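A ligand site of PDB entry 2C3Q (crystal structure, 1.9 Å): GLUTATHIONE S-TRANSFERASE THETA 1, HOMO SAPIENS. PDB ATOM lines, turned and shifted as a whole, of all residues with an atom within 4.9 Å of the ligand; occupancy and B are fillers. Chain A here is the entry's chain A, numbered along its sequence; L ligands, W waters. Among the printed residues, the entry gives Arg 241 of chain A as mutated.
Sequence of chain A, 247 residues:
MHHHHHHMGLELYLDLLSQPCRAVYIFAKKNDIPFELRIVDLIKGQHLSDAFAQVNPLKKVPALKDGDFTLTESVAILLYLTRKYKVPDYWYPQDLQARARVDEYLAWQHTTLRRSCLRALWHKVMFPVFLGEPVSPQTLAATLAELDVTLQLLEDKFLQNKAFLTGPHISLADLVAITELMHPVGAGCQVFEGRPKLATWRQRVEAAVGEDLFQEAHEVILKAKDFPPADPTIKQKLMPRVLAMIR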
ATOM      1  N   LEU A  17     -18.710 -26.507 -23.201  1.00  0.00           N
ATOM      2  CA  LEU A  17     -18.362 -25.443 -24.099  1.00  0.00           C
ATOM      3  C   LEU A  17     -16.968 -25.718 -24.725  1.00  0.00           C
ATOM      4  O   LEU A  17     -16.771 -25.428 -25.900  1.00  0.00           O
ATOM      5  CB  LEU A  17     -18.366 -24.084 -23.384  1.00  0.00           C
ATOM      6  CG  LEU A  17     -17.780 -22.862 -24.106  1.00  0.00           C
ATOM      7  CD1 LEU A  17     -18.567 -22.510 -25.399  1.00  0.00           C
ATOM      8  CD2 LEU A  17     -17.702 -21.673 -23.172  1.00  0.00           C
ATOM      9  N   SER A  18     -16.042 -26.316 -23.964  1.00  0.00           N
ATOM     10  CA  SER A  18     -14.664 -26.529 -24.463  1.00  0.00           C
ATOM     11  C   SER A  18     -14.469 -27.843 -25.236  1.00  0.00           C
ATOM     12  O   SER A  18     -15.037 -28.866 -24.850  1.00  0.00           O
ATOM     13  CB  SER A  18     -13.656 -26.455 -23.308  1.00  0.00           C
ATOM     14  OG  SER A  18     -13.462 -27.681 -22.679  1.00  0.00           O
ATOM     15  N   PRO A  20     -11.717 -29.942 -25.507  1.00  0.00           N
ATOM     16  CA  PRO A  20     -11.186 -31.134 -24.809  1.00  0.00           C
ATOM     17  C   PRO A  20     -12.153 -31.820 -23.842  1.00  0.00           C
ATOM     18  O   PRO A  20     -12.101 -33.037 -23.708  1.00  0.00           O
ATOM     19  CB  PRO A  20      -9.969 -30.559 -24.045  1.00  0.00           C
ATOM     20  CG  PRO A  20     -10.228 -29.126 -23.890  1.00  0.00           C
ATOM     21  CD  PRO A  20     -10.909 -28.752 -25.144  1.00  0.00           C
ATOM     22  N   LEU A  42     -17.220 -21.954 -17.095  1.00  0.00           N
ATOM     23  CA  LEU A  42     -16.169 -21.066 -17.607  1.00  0.00           C
ATOM     24  C   LEU A  42     -16.624 -19.608 -17.760  1.00  0.00           C
ATOM     25  O   LEU A  42     -15.908 -18.681 -17.359  1.00  0.00           O
ATOM     26  CB  LEU A  42     -15.619 -21.583 -18.961  1.00  0.00           C
ATOM     27  CG  LEU A  42     -14.885 -22.925 -18.975  1.00  0.00           C
ATOM     28  CD1 LEU A  42     -14.738 -23.477 -20.424  1.00  0.00           C
ATOM     29  CD2 LEU A  42     -13.544 -22.802 -18.262  1.00  0.00           C
ATOM     30  N   ILE A  43     -17.831 -19.470 -18.328  1.00  0.00           N
ATOM     31  CA  ILE A  43     -18.563 -18.210 -18.575  1.00  0.00           C
ATOM     32  C   ILE A  43     -18.766 -17.356 -17.307  1.00  0.00           C
ATOM     33  O   ILE A  43     -18.772 -16.114 -17.366  1.00  0.00           O
ATOM     34  CB  ILE A  43     -19.893 -18.590 -19.374  1.00  0.00           C
ATOM     35  CG1 ILE A  43     -19.769 -18.230 -20.842  1.00  0.00           C
ATOM     36  CG2 ILE A  43     -21.154 -17.910 -18.909  1.00  0.00           C
ATOM     37  CD1 ILE A  43     -18.511 -18.516 -21.473  1.00  0.00           C
ATOM     38  N   HIS A  47     -13.845 -21.662 -12.952  1.00  0.00           N
ATOM     39  CA  HIS A  47     -12.494 -22.253 -13.009  1.00  0.00           C
ATOM     40  C   HIS A  47     -11.412 -21.400 -12.287  1.00  0.00           C
ATOM     41  O   HIS A  47     -10.340 -21.905 -11.963  1.00  0.00           O
ATOM     42  CB  HIS A  47     -12.108 -22.535 -14.461  1.00  0.00           C
ATOM     43  CG  HIS A  47     -12.006 -21.323 -15.326  1.00  0.00           C
ATOM     44  ND1 HIS A  47     -13.097 -20.545 -15.674  1.00  0.00           N
ATOM     45  CD2 HIS A  47     -10.954 -20.790 -15.989  1.00  0.00           C
ATOM     46  CE1 HIS A  47     -12.703 -19.575 -16.473  1.00  0.00           C
ATOM     47  NE2 HIS A  47     -11.414 -19.695 -16.687  1.00  0.00           N
ATOM     48  N   LEU A  48     -11.728 -20.132 -12.017  1.00  0.00           N
ATOM     49  CA  LEU A  48     -10.823 -19.194 -11.335  1.00  0.00           C
ATOM     50  C   LEU A  48     -11.084 -19.102  -9.822  1.00  0.00           C
ATOM     51  O   LEU A  48     -10.364 -18.399  -9.101  1.00  0.00           O
ATOM     52  CB  LEU A  48     -10.917 -17.802 -11.974  1.00  0.00           C
ATOM     53  CG  LEU A  48     -10.764 -17.744 -13.493  1.00  0.00           C
ATOM     54  CD1 LEU A  48     -11.054 -16.345 -14.026  1.00  0.00           C
ATOM     55  CD2 LEU A  48      -9.362 -18.219 -13.961  1.00  0.00           C
ATOM     56  N   LYS A  59      -5.919 -23.924 -13.295  1.00  0.00           N
ATOM     57  CA  LYS A  59      -7.259 -23.285 -13.474  1.00  0.00           C
ATOM     58  C   LYS A  59      -7.833 -23.550 -14.879  1.00  0.00           C
ATOM     59  O   LYS A  59      -8.363 -22.653 -15.562  1.00  0.00           O
ATOM     60  CB  LYS A  59      -7.216 -21.776 -13.165  1.00  0.00           C
ATOM     61  CG  LYS A  59      -6.713 -21.403 -11.763  1.00  0.00           C
ATOM     62  CD  LYS A  59      -6.339 -19.926 -11.757  1.00  0.00           C
ATOM     63  CE  LYS A  59      -5.639 -19.470 -10.468  1.00  0.00           C
ATOM     64  NZ  LYS A  59      -6.519 -19.565  -9.280  1.00  0.00           N
ATOM     65  N   LYS A  60      -7.701 -24.798 -15.294  1.00  0.00           N
ATOM     66  CA  LYS A  60      -8.186 -25.203 -16.610  1.00  0.00           C
ATOM     67  C   LYS A  60      -9.003 -26.480 -16.552  1.00  0.00           C
ATOM     68  O   LYS A  60      -8.869 -27.306 -15.635  1.00  0.00           O
ATOM     69  CB  LYS A  60      -6.992 -25.373 -17.558  1.00  0.00           C
ATOM     70  CG  LYS A  60      -6.383 -24.065 -17.986  1.00  0.00           C
ATOM     71  CD  LYS A  60      -5.089 -24.256 -18.731  1.00  0.00           C
ATOM     72  CE  LYS A  60      -4.489 -22.912 -19.140  1.00  0.00           C
ATOM     73  NZ  LYS A  60      -5.170 -22.285 -20.279  1.00  0.00           N
ATOM     74  N   VAL A  61      -9.843 -26.657 -17.571  1.00  0.00           N
ATOM     75  CA  VAL A  61     -10.626 -27.876 -17.695  1.00  0.00           C
ATOM     76  C   VAL A  61     -10.240 -28.559 -19.011  1.00  0.00           C
ATOM     77  O   VAL A  61      -9.840 -27.860 -19.957  1.00  0.00           O
ATOM     78  CB  VAL A  61     -12.189 -27.638 -17.587  1.00  0.00           C
ATOM     79  CG1 VAL A  61     -12.602 -27.342 -16.126  1.00  0.00           C
ATOM     80  CG2 VAL A  61     -12.664 -26.546 -18.565  1.00  0.00           C
ATOM     81  N   PRO A  62     -10.345 -29.910 -19.103  1.00  0.00           N
ATOM     82  CA  PRO A  62     -10.775 -30.975 -18.192  1.00  0.00           C
ATOM     83  C   PRO A  62      -9.764 -31.276 -17.095  1.00  0.00           C
ATOM     84  O   PRO A  62      -8.562 -31.064 -17.282  1.00  0.00           O
ATOM     85  CB  PRO A  62     -10.880 -32.197 -19.097  1.00  0.00           C
ATOM     86  CG  PRO A  62      -9.936 -31.941 -20.190  1.00  0.00           C
ATOM     87  CD  PRO A  62      -9.958 -30.467 -20.411  1.00  0.00           C
ATOM     88  N   GLU A  73      -4.915 -32.530 -18.812  1.00  0.00           N
ATOM     89  CA  GLU A  73      -4.685 -32.778 -20.258  1.00  0.00           C
ATOM     90  C   GLU A  73      -5.631 -33.831 -20.777  1.00  0.00           C
ATOM     91  O   GLU A  73      -5.566 -34.984 -20.363  1.00  0.00           O
ATOM     92  CB  GLU A  73      -3.213 -33.149 -20.567  1.00  0.00           C
ATOM     93  CG  GLU A  73      -2.219 -32.016 -20.261  1.00  0.00           C
ATOM     94  CD  GLU A  73      -2.397 -30.830 -21.188  1.00  0.00           C
ATOM     95  OE1 GLU A  73      -2.734 -31.013 -22.391  1.00  0.00           O
ATOM     96  OE2 GLU A  73      -2.159 -29.706 -20.753  1.00  0.00           O
ATOM     97  N   SER A  74      -6.536 -33.440 -21.672  1.00  0.00           N
ATOM     98  CA  SER A  74      -7.499 -34.390 -22.249  1.00  0.00           C
ATOM     99  C   SER A  74      -6.842 -35.636 -22.848  1.00  0.00           C
ATOM    100  O   SER A  74      -7.371 -36.694 -22.649  1.00  0.00           O
ATOM    101  CB  SER A  74      -8.362 -33.738 -23.336  1.00  0.00           C
ATOM    102  OG  SER A  74      -7.529 -33.142 -24.327  1.00  0.00           O
ATOM    103  N   VAL A  75      -5.677 -35.524 -23.520  1.00  0.00           N
ATOM    104  CA  VAL A  75      -5.035 -36.727 -24.121  1.00  0.00           C
ATOM    105  C   VAL A  75      -4.636 -37.699 -23.000  1.00  0.00           C
ATOM    106  O   VAL A  75      -4.898 -38.900 -23.110  1.00  0.00           O
ATOM    107  CB  VAL A  75      -3.872 -36.361 -25.120  1.00  0.00           C
ATOM    108  CG1 VAL A  75      -3.043 -37.588 -25.542  1.00  0.00           C
ATOM    109  CG2 VAL A  75      -4.454 -35.652 -26.318  1.00  0.00           C
ATOM    110  N   HIS A 110      -2.451 -30.691 -31.335  1.00  0.00           N
ATOM    111  CA  HIS A 110      -2.263 -29.694 -30.265  1.00  0.00           C
ATOM    112  C   HIS A 110      -1.915 -28.286 -30.788  1.00  0.00           C
ATOM    113  O   HIS A 110      -2.499 -27.306 -30.334  1.00  0.00           O
ATOM    114  CB  HIS A 110      -1.158 -30.103 -29.298  1.00  0.00           C
ATOM    115  CG  HIS A 110      -1.496 -31.264 -28.419  1.00  0.00           C
ATOM    116  ND1 HIS A 110      -2.414 -31.198 -27.391  1.00  0.00           N
ATOM    117  CD2 HIS A 110      -0.978 -32.511 -28.359  1.00  0.00           C
ATOM    118  CE1 HIS A 110      -2.480 -32.359 -26.785  1.00  0.00           C
ATOM    119  NE2 HIS A 110      -1.597 -33.179 -27.346  1.00  0.00           N
ATOM    120  N   LEU A 118     -10.062 -23.380 -31.937  1.00  0.00           N
ATOM    121  CA  LEU A 118     -10.241 -22.493 -30.785  1.00  0.00           C
ATOM    122  C   LEU A 118     -10.252 -21.005 -31.203  1.00  0.00           C
ATOM    123  O   LEU A 118     -11.104 -20.229 -30.735  1.00  0.00           O
ATOM    124  CB  LEU A 118      -9.175 -22.731 -29.714  1.00  0.00           C
ATOM    125  CG  LEU A 118      -9.184 -21.835 -28.472  1.00  0.00           C
ATOM    126  CD1 LEU A 118     -10.326 -22.165 -27.489  1.00  0.00           C
ATOM    127  CD2 LEU A 118      -7.845 -21.919 -27.761  1.00  0.00           C
ATOM    128  N   TRP A 122     -13.358 -17.971 -31.000  1.00  0.00           N
ATOM    129  CA  TRP A 122     -13.099 -16.687 -30.307  1.00  0.00           C
ATOM    130  C   TRP A 122     -13.078 -15.474 -31.237  1.00  0.00           C
ATOM    131  O   TRP A 122     -13.717 -14.472 -30.929  1.00  0.00           O
ATOM    132  CB  TRP A 122     -11.803 -16.785 -29.452  1.00  0.00           C
ATOM    133  CG  TRP A 122     -12.186 -17.534 -28.226  1.00  0.00           C
ATOM    134  CD1 TRP A 122     -12.221 -18.892 -28.059  1.00  0.00           C
ATOM    135  CD2 TRP A 122     -12.740 -16.971 -27.035  1.00  0.00           C
ATOM    136  NE1 TRP A 122     -12.753 -19.218 -26.832  1.00  0.00           N
ATOM    137  CE2 TRP A 122     -13.085 -18.045 -26.182  1.00  0.00           C
ATOM    138  CE3 TRP A 122     -12.981 -15.649 -26.599  1.00  0.00           C
ATOM    139  CZ2 TRP A 122     -13.646 -17.856 -24.912  1.00  0.00           C
ATOM    140  CZ3 TRP A 122     -13.577 -15.458 -25.337  1.00  0.00           C
ATOM    141  CH2 TRP A 122     -13.882 -16.561 -24.506  1.00  0.00           C
ATOM    142  N   MET A 126     -16.942 -15.491 -29.779  1.00  0.00           N
ATOM    143  CA  MET A 126     -16.827 -15.289 -28.296  1.00  0.00           C
ATOM    144  C   MET A 126     -16.206 -13.933 -27.897  1.00  0.00           C
ATOM    145  O   MET A 126     -16.585 -13.402 -26.830  1.00  0.00           O
ATOM    146  CB  MET A 126     -16.092 -16.461 -27.669  1.00  0.00           C
ATOM    147  CG  MET A 126     -16.851 -17.779 -27.640  1.00  0.00           C
ATOM    148  SD  MET A 126     -18.322 -17.854 -26.632  1.00  0.00           S
ATOM    149  CE  MET A 126     -17.595 -17.670 -25.000  1.00  0.00           C
ATOM    150  N   PHE A 130     -19.758 -12.493 -26.580  1.00  0.00           N
ATOM    151  CA  PHE A 130     -19.670 -12.689 -25.138  1.00  0.00           C
ATOM    152  C   PHE A 130     -18.803 -11.612 -24.446  1.00  0.00           C
ATOM    153  O   PHE A 130     -19.191 -11.094 -23.395  1.00  0.00           O
ATOM    154  CB  PHE A 130     -19.161 -14.107 -24.840  1.00  0.00           C
ATOM    155  CG  PHE A 130     -18.900 -14.358 -23.406  1.00  0.00           C
ATOM    156  CD1 PHE A 130     -19.962 -14.369 -22.489  1.00  0.00           C
ATOM    157  CD2 PHE A 130     -17.613 -14.591 -22.953  1.00  0.00           C
ATOM    158  CE1 PHE A 130     -19.737 -14.600 -21.155  1.00  0.00           C
ATOM    159  CE2 PHE A 130     -17.376 -14.841 -21.609  1.00  0.00           C
ATOM    160  CZ  PHE A 130     -18.432 -14.845 -20.707  1.00  0.00           C
ATOM    161  N   LEU A 238     -11.779 -12.521 -16.877  1.00  0.00           N
ATOM    162  CA  LEU A 238     -11.539 -13.496 -17.948  1.00  0.00           C
ATOM    163  C   LEU A 238     -10.630 -12.996 -19.064  1.00  0.00           C
ATOM    164  O   LEU A 238      -9.976 -13.823 -19.680  1.00  0.00           O
ATOM    165  CB  LEU A 238     -12.863 -13.963 -18.588  1.00  0.00           C
ATOM    166  CG  LEU A 238     -13.916 -14.730 -17.777  1.00  0.00           C
ATOM    167  CD1 LEU A 238     -15.076 -15.005 -18.738  1.00  0.00           C
ATOM    168  CD2 LEU A 238     -13.446 -16.033 -17.131  1.00  0.00           C
ATOM    169  N   ARG A 241      -6.954 -14.232 -19.067  1.00  0.00           N
ATOM    170  CA  ARG A 241      -7.022 -15.681 -19.300  1.00  0.00           C
ATOM    171  C   ARG A 241      -7.262 -16.015 -20.769  1.00  0.00           C
ATOM    172  O   ARG A 241      -6.640 -16.918 -21.322  1.00  0.00           O
ATOM    173  CB  ARG A 241      -8.137 -16.317 -18.478  1.00  0.00           C
ATOM    174  CG  ARG A 241      -8.049 -16.167 -16.961  1.00  0.00           C
ATOM    175  CD  ARG A 241      -6.817 -16.816 -16.367  1.00  0.00           C
ATOM    176  NE  ARG A 241      -6.816 -18.263 -16.618  1.00  0.00           N
ATOM    177  CZ  ARG A 241      -5.950 -19.127 -16.088  1.00  0.00           C
ATOM    178  NH1 ARG A 241      -5.003 -18.721 -15.251  1.00  0.00           N
ATOM    179  NH2 ARG A 241      -6.053 -20.405 -16.396  1.00  0.00           N
ATOM    180  N   VAL A 242      -8.182 -15.270 -21.385  1.00  0.00           N
ATOM    181  CA  VAL A 242      -8.517 -15.452 -22.799  1.00  0.00           C
ATOM    182  C   VAL A 242      -7.331 -15.026 -23.710  1.00  0.00           C
ATOM    183  O   VAL A 242      -7.036 -15.733 -24.670  1.00  0.00           O
ATOM    184  CB  VAL A 242      -9.860 -14.733 -23.126  1.00  0.00           C
ATOM    185  CG1 VAL A 242     -10.112 -14.685 -24.590  1.00  0.00           C
ATOM    186  CG2 VAL A 242     -11.010 -15.450 -22.439  1.00  0.00           C
ATOM    187  N   MET A 245      -4.751 -17.644 -23.790  1.00  0.00           N
ATOM    188  CA  MET A 245      -5.320 -18.719 -24.557  1.00  0.00           C
ATOM    189  C   MET A 245      -5.241 -18.415 -26.060  1.00  0.00           C
ATOM    190  O   MET A 245      -4.836 -19.265 -26.852  1.00  0.00           O
ATOM    191  CB  MET A 245      -6.767 -18.910 -24.091  1.00  0.00           C
ATOM    192  CG  MET A 245      -7.359 -20.239 -24.320  1.00  0.00           C
ATOM    193  SD  MET A 245      -6.683 -21.411 -23.135  1.00  0.00           S
ATOM    194  CE  MET A 245      -6.873 -22.790 -24.216  1.00  0.00           C
HETATM  195  N1  LIG L   1      -4.152 -29.007 -23.621  1.00  0.00           N
HETATM  196  C1  LIG L   1      -5.215 -28.915 -22.614  1.00  0.00           C
HETATM  197  C2  LIG L   1      -6.108 -30.116 -22.694  1.00  0.00           C
HETATM  198  O1  LIG L   1      -6.233 -30.722 -23.792  1.00  0.00           O
HETATM  199  O2  LIG L   1      -6.739 -30.507 -21.688  1.00  0.00           O
HETATM  200  C3  LIG L   1      -6.046 -27.656 -22.807  1.00  0.00           C
HETATM  201  C4  LIG L   1      -6.538 -27.244 -21.402  1.00  0.00           C
HETATM  202  C5  LIG L   1      -7.175 -25.891 -21.531  1.00  0.00           C
HETATM  203  O3  LIG L   1      -6.358 -24.845 -21.875  1.00  0.00           O
HETATM  204  N2  LIG L   1      -8.458 -25.753 -21.280  1.00  0.00           N
HETATM  205  C6  LIG L   1      -9.117 -24.491 -21.537  1.00  0.00           C
HETATM  206  C7  LIG L   1      -9.424 -23.743 -20.269  1.00  0.00           C
HETATM  207  O4  LIG L   1     -10.044 -24.406 -19.235  1.00  0.00           O
HETATM  208  C8  LIG L   1     -10.363 -24.815 -22.339  1.00  0.00           C
HETATM  209  S1  LIG L   1     -11.632 -23.537 -22.357  1.00  0.00           S
HETATM  210  C9  LIG L   1     -10.764 -22.322 -23.377  1.00  0.00           C
HETATM  211  C10 LIG L   1     -11.262 -20.867 -23.200  1.00  0.00           C
HETATM  212  C11 LIG L   1     -11.787 -20.496 -21.806  1.00  0.00           C
HETATM  213  C12 LIG L   1     -12.291 -19.052 -21.723  1.00  0.00           C
HETATM  214  C13 LIG L   1     -13.359 -18.873 -20.653  1.00  0.00           C
HETATM  215  C14 LIG L   1     -14.709 -18.517 -21.259  1.00  0.00           C
HETATM  216  N3  LIG L   1      -9.090 -22.470 -20.227  1.00  0.00           N
HETATM  217  C15 LIG L   1      -9.373 -21.655 -19.061  1.00  0.00           C
HETATM  218  C16 LIG L   1      -8.338 -20.590 -18.815  1.00  0.00           C
HETATM  219  O5  LIG L   1      -8.671 -19.589 -18.152  1.00  0.00           O
HETATM  220  O6  LIG L   1      -7.190 -20.672 -19.263  1.00  0.00           O
HETATM  221  O   HOH W   1      -4.310 -32.837 -24.166  1.00  0.00           O
HETATM  222  O   HOH W   2      -6.526 -30.101 -18.902  1.00  0.00           O
HETATM  223  O   HOH W   3      -3.106 -26.534 -24.574  1.00  0.00           O
HETATM  224  O   HOH W   4      -5.354 -18.755 -19.758  1.00  0.00           O
HETATM  225  O   HOH W   5      -4.579 -29.815 -26.344  1.00  0.00           O
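O3 of the ligand sits close to SD of Met 245, at 3.7 Å. Residues that only touch the ligand: Ser 18 (3.7 Å), Pro 20 (3.7 Å), Leu 42 (3.7 Å), Ile 43 (3.8 Å), Lys 59 (3.8 Å), Pro 62 (3.5 Å), Trp 122 (3.7 Å) and Val 242 (3.9 Å). 15 residues have an atom within 4 Å of the ligand: Ser 18, Pro 20, Leu 42, Ile 43, His 47, Lys 59, Lys 60, Val 61, Pro 62, Glu 73, Ser 74, Trp 122, Arg 241, Val 242 and Met 245.
Water W4 bridges an oxygen (O6) of the ligand (2.7 Å) and the backbone carbonyl oxygen (O) of Arg 241 (2.7 Å). Water W2 lies within hydrogen-bond range of O of Pro 62, O2 of the ligand and N of Glu 73. Water W5 lies within hydrogen-bond range of a ring nitrogen (ND1) of His 110 and a nitrogen (N1) of the ligand. Water W1 lies within hydrogen-bond range of an oxygen (O1) of the ligand (2.9 Å), the side-chain carboxylate (OE1) of Glu 73 (3.0 Å), the backbone NH (N) of Val 75 (3.1 Å) and the side-chain hydroxyl (OG) of Ser 74 (3.2 Å).
The backbone NH (N) of Ser 74 sits at hydrogen-bond distance from an oxygen (O2) of the ligand. The guanidinium group of Arg 241 lies within salt-bridge range of an oxygen (O5) of the ligand, at 2.7 Å. N of Val 61 lies within hydrogen-bond range of O4 of the ligand. The side-chain hydroxyl (OG) of Ser 74 is in hydrogen-bond range of an oxygen (O1) of the ligand (2.8 Å). The backbone carbonyl oxygen (O) of Val 61 is in hydrogen-bond range of a nitrogen (N2) of the ligand (2.8 Å). The side-chain carboxylate (OE1) of Glu 73 is in salt-bridge range of a nitrogen (N1) of the ligand (2.7 Å). NZ of Lys 60 is in salt-bridge range of O6 of the ligand, 2.8 Å away. A ring nitrogen (NE2) of His 47 lies within hydrogen-bond range of an oxygen (O5) of the ligand, at 3.1 Å.
The side-chain amino group of Lys 60 is in hydrogen-bond range of the side-chain sulfur of Met 245 (3.3 Å). O of Lys 59 lies within hydrogen-bond range of NH2 of Arg 241 (3.3 Å).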
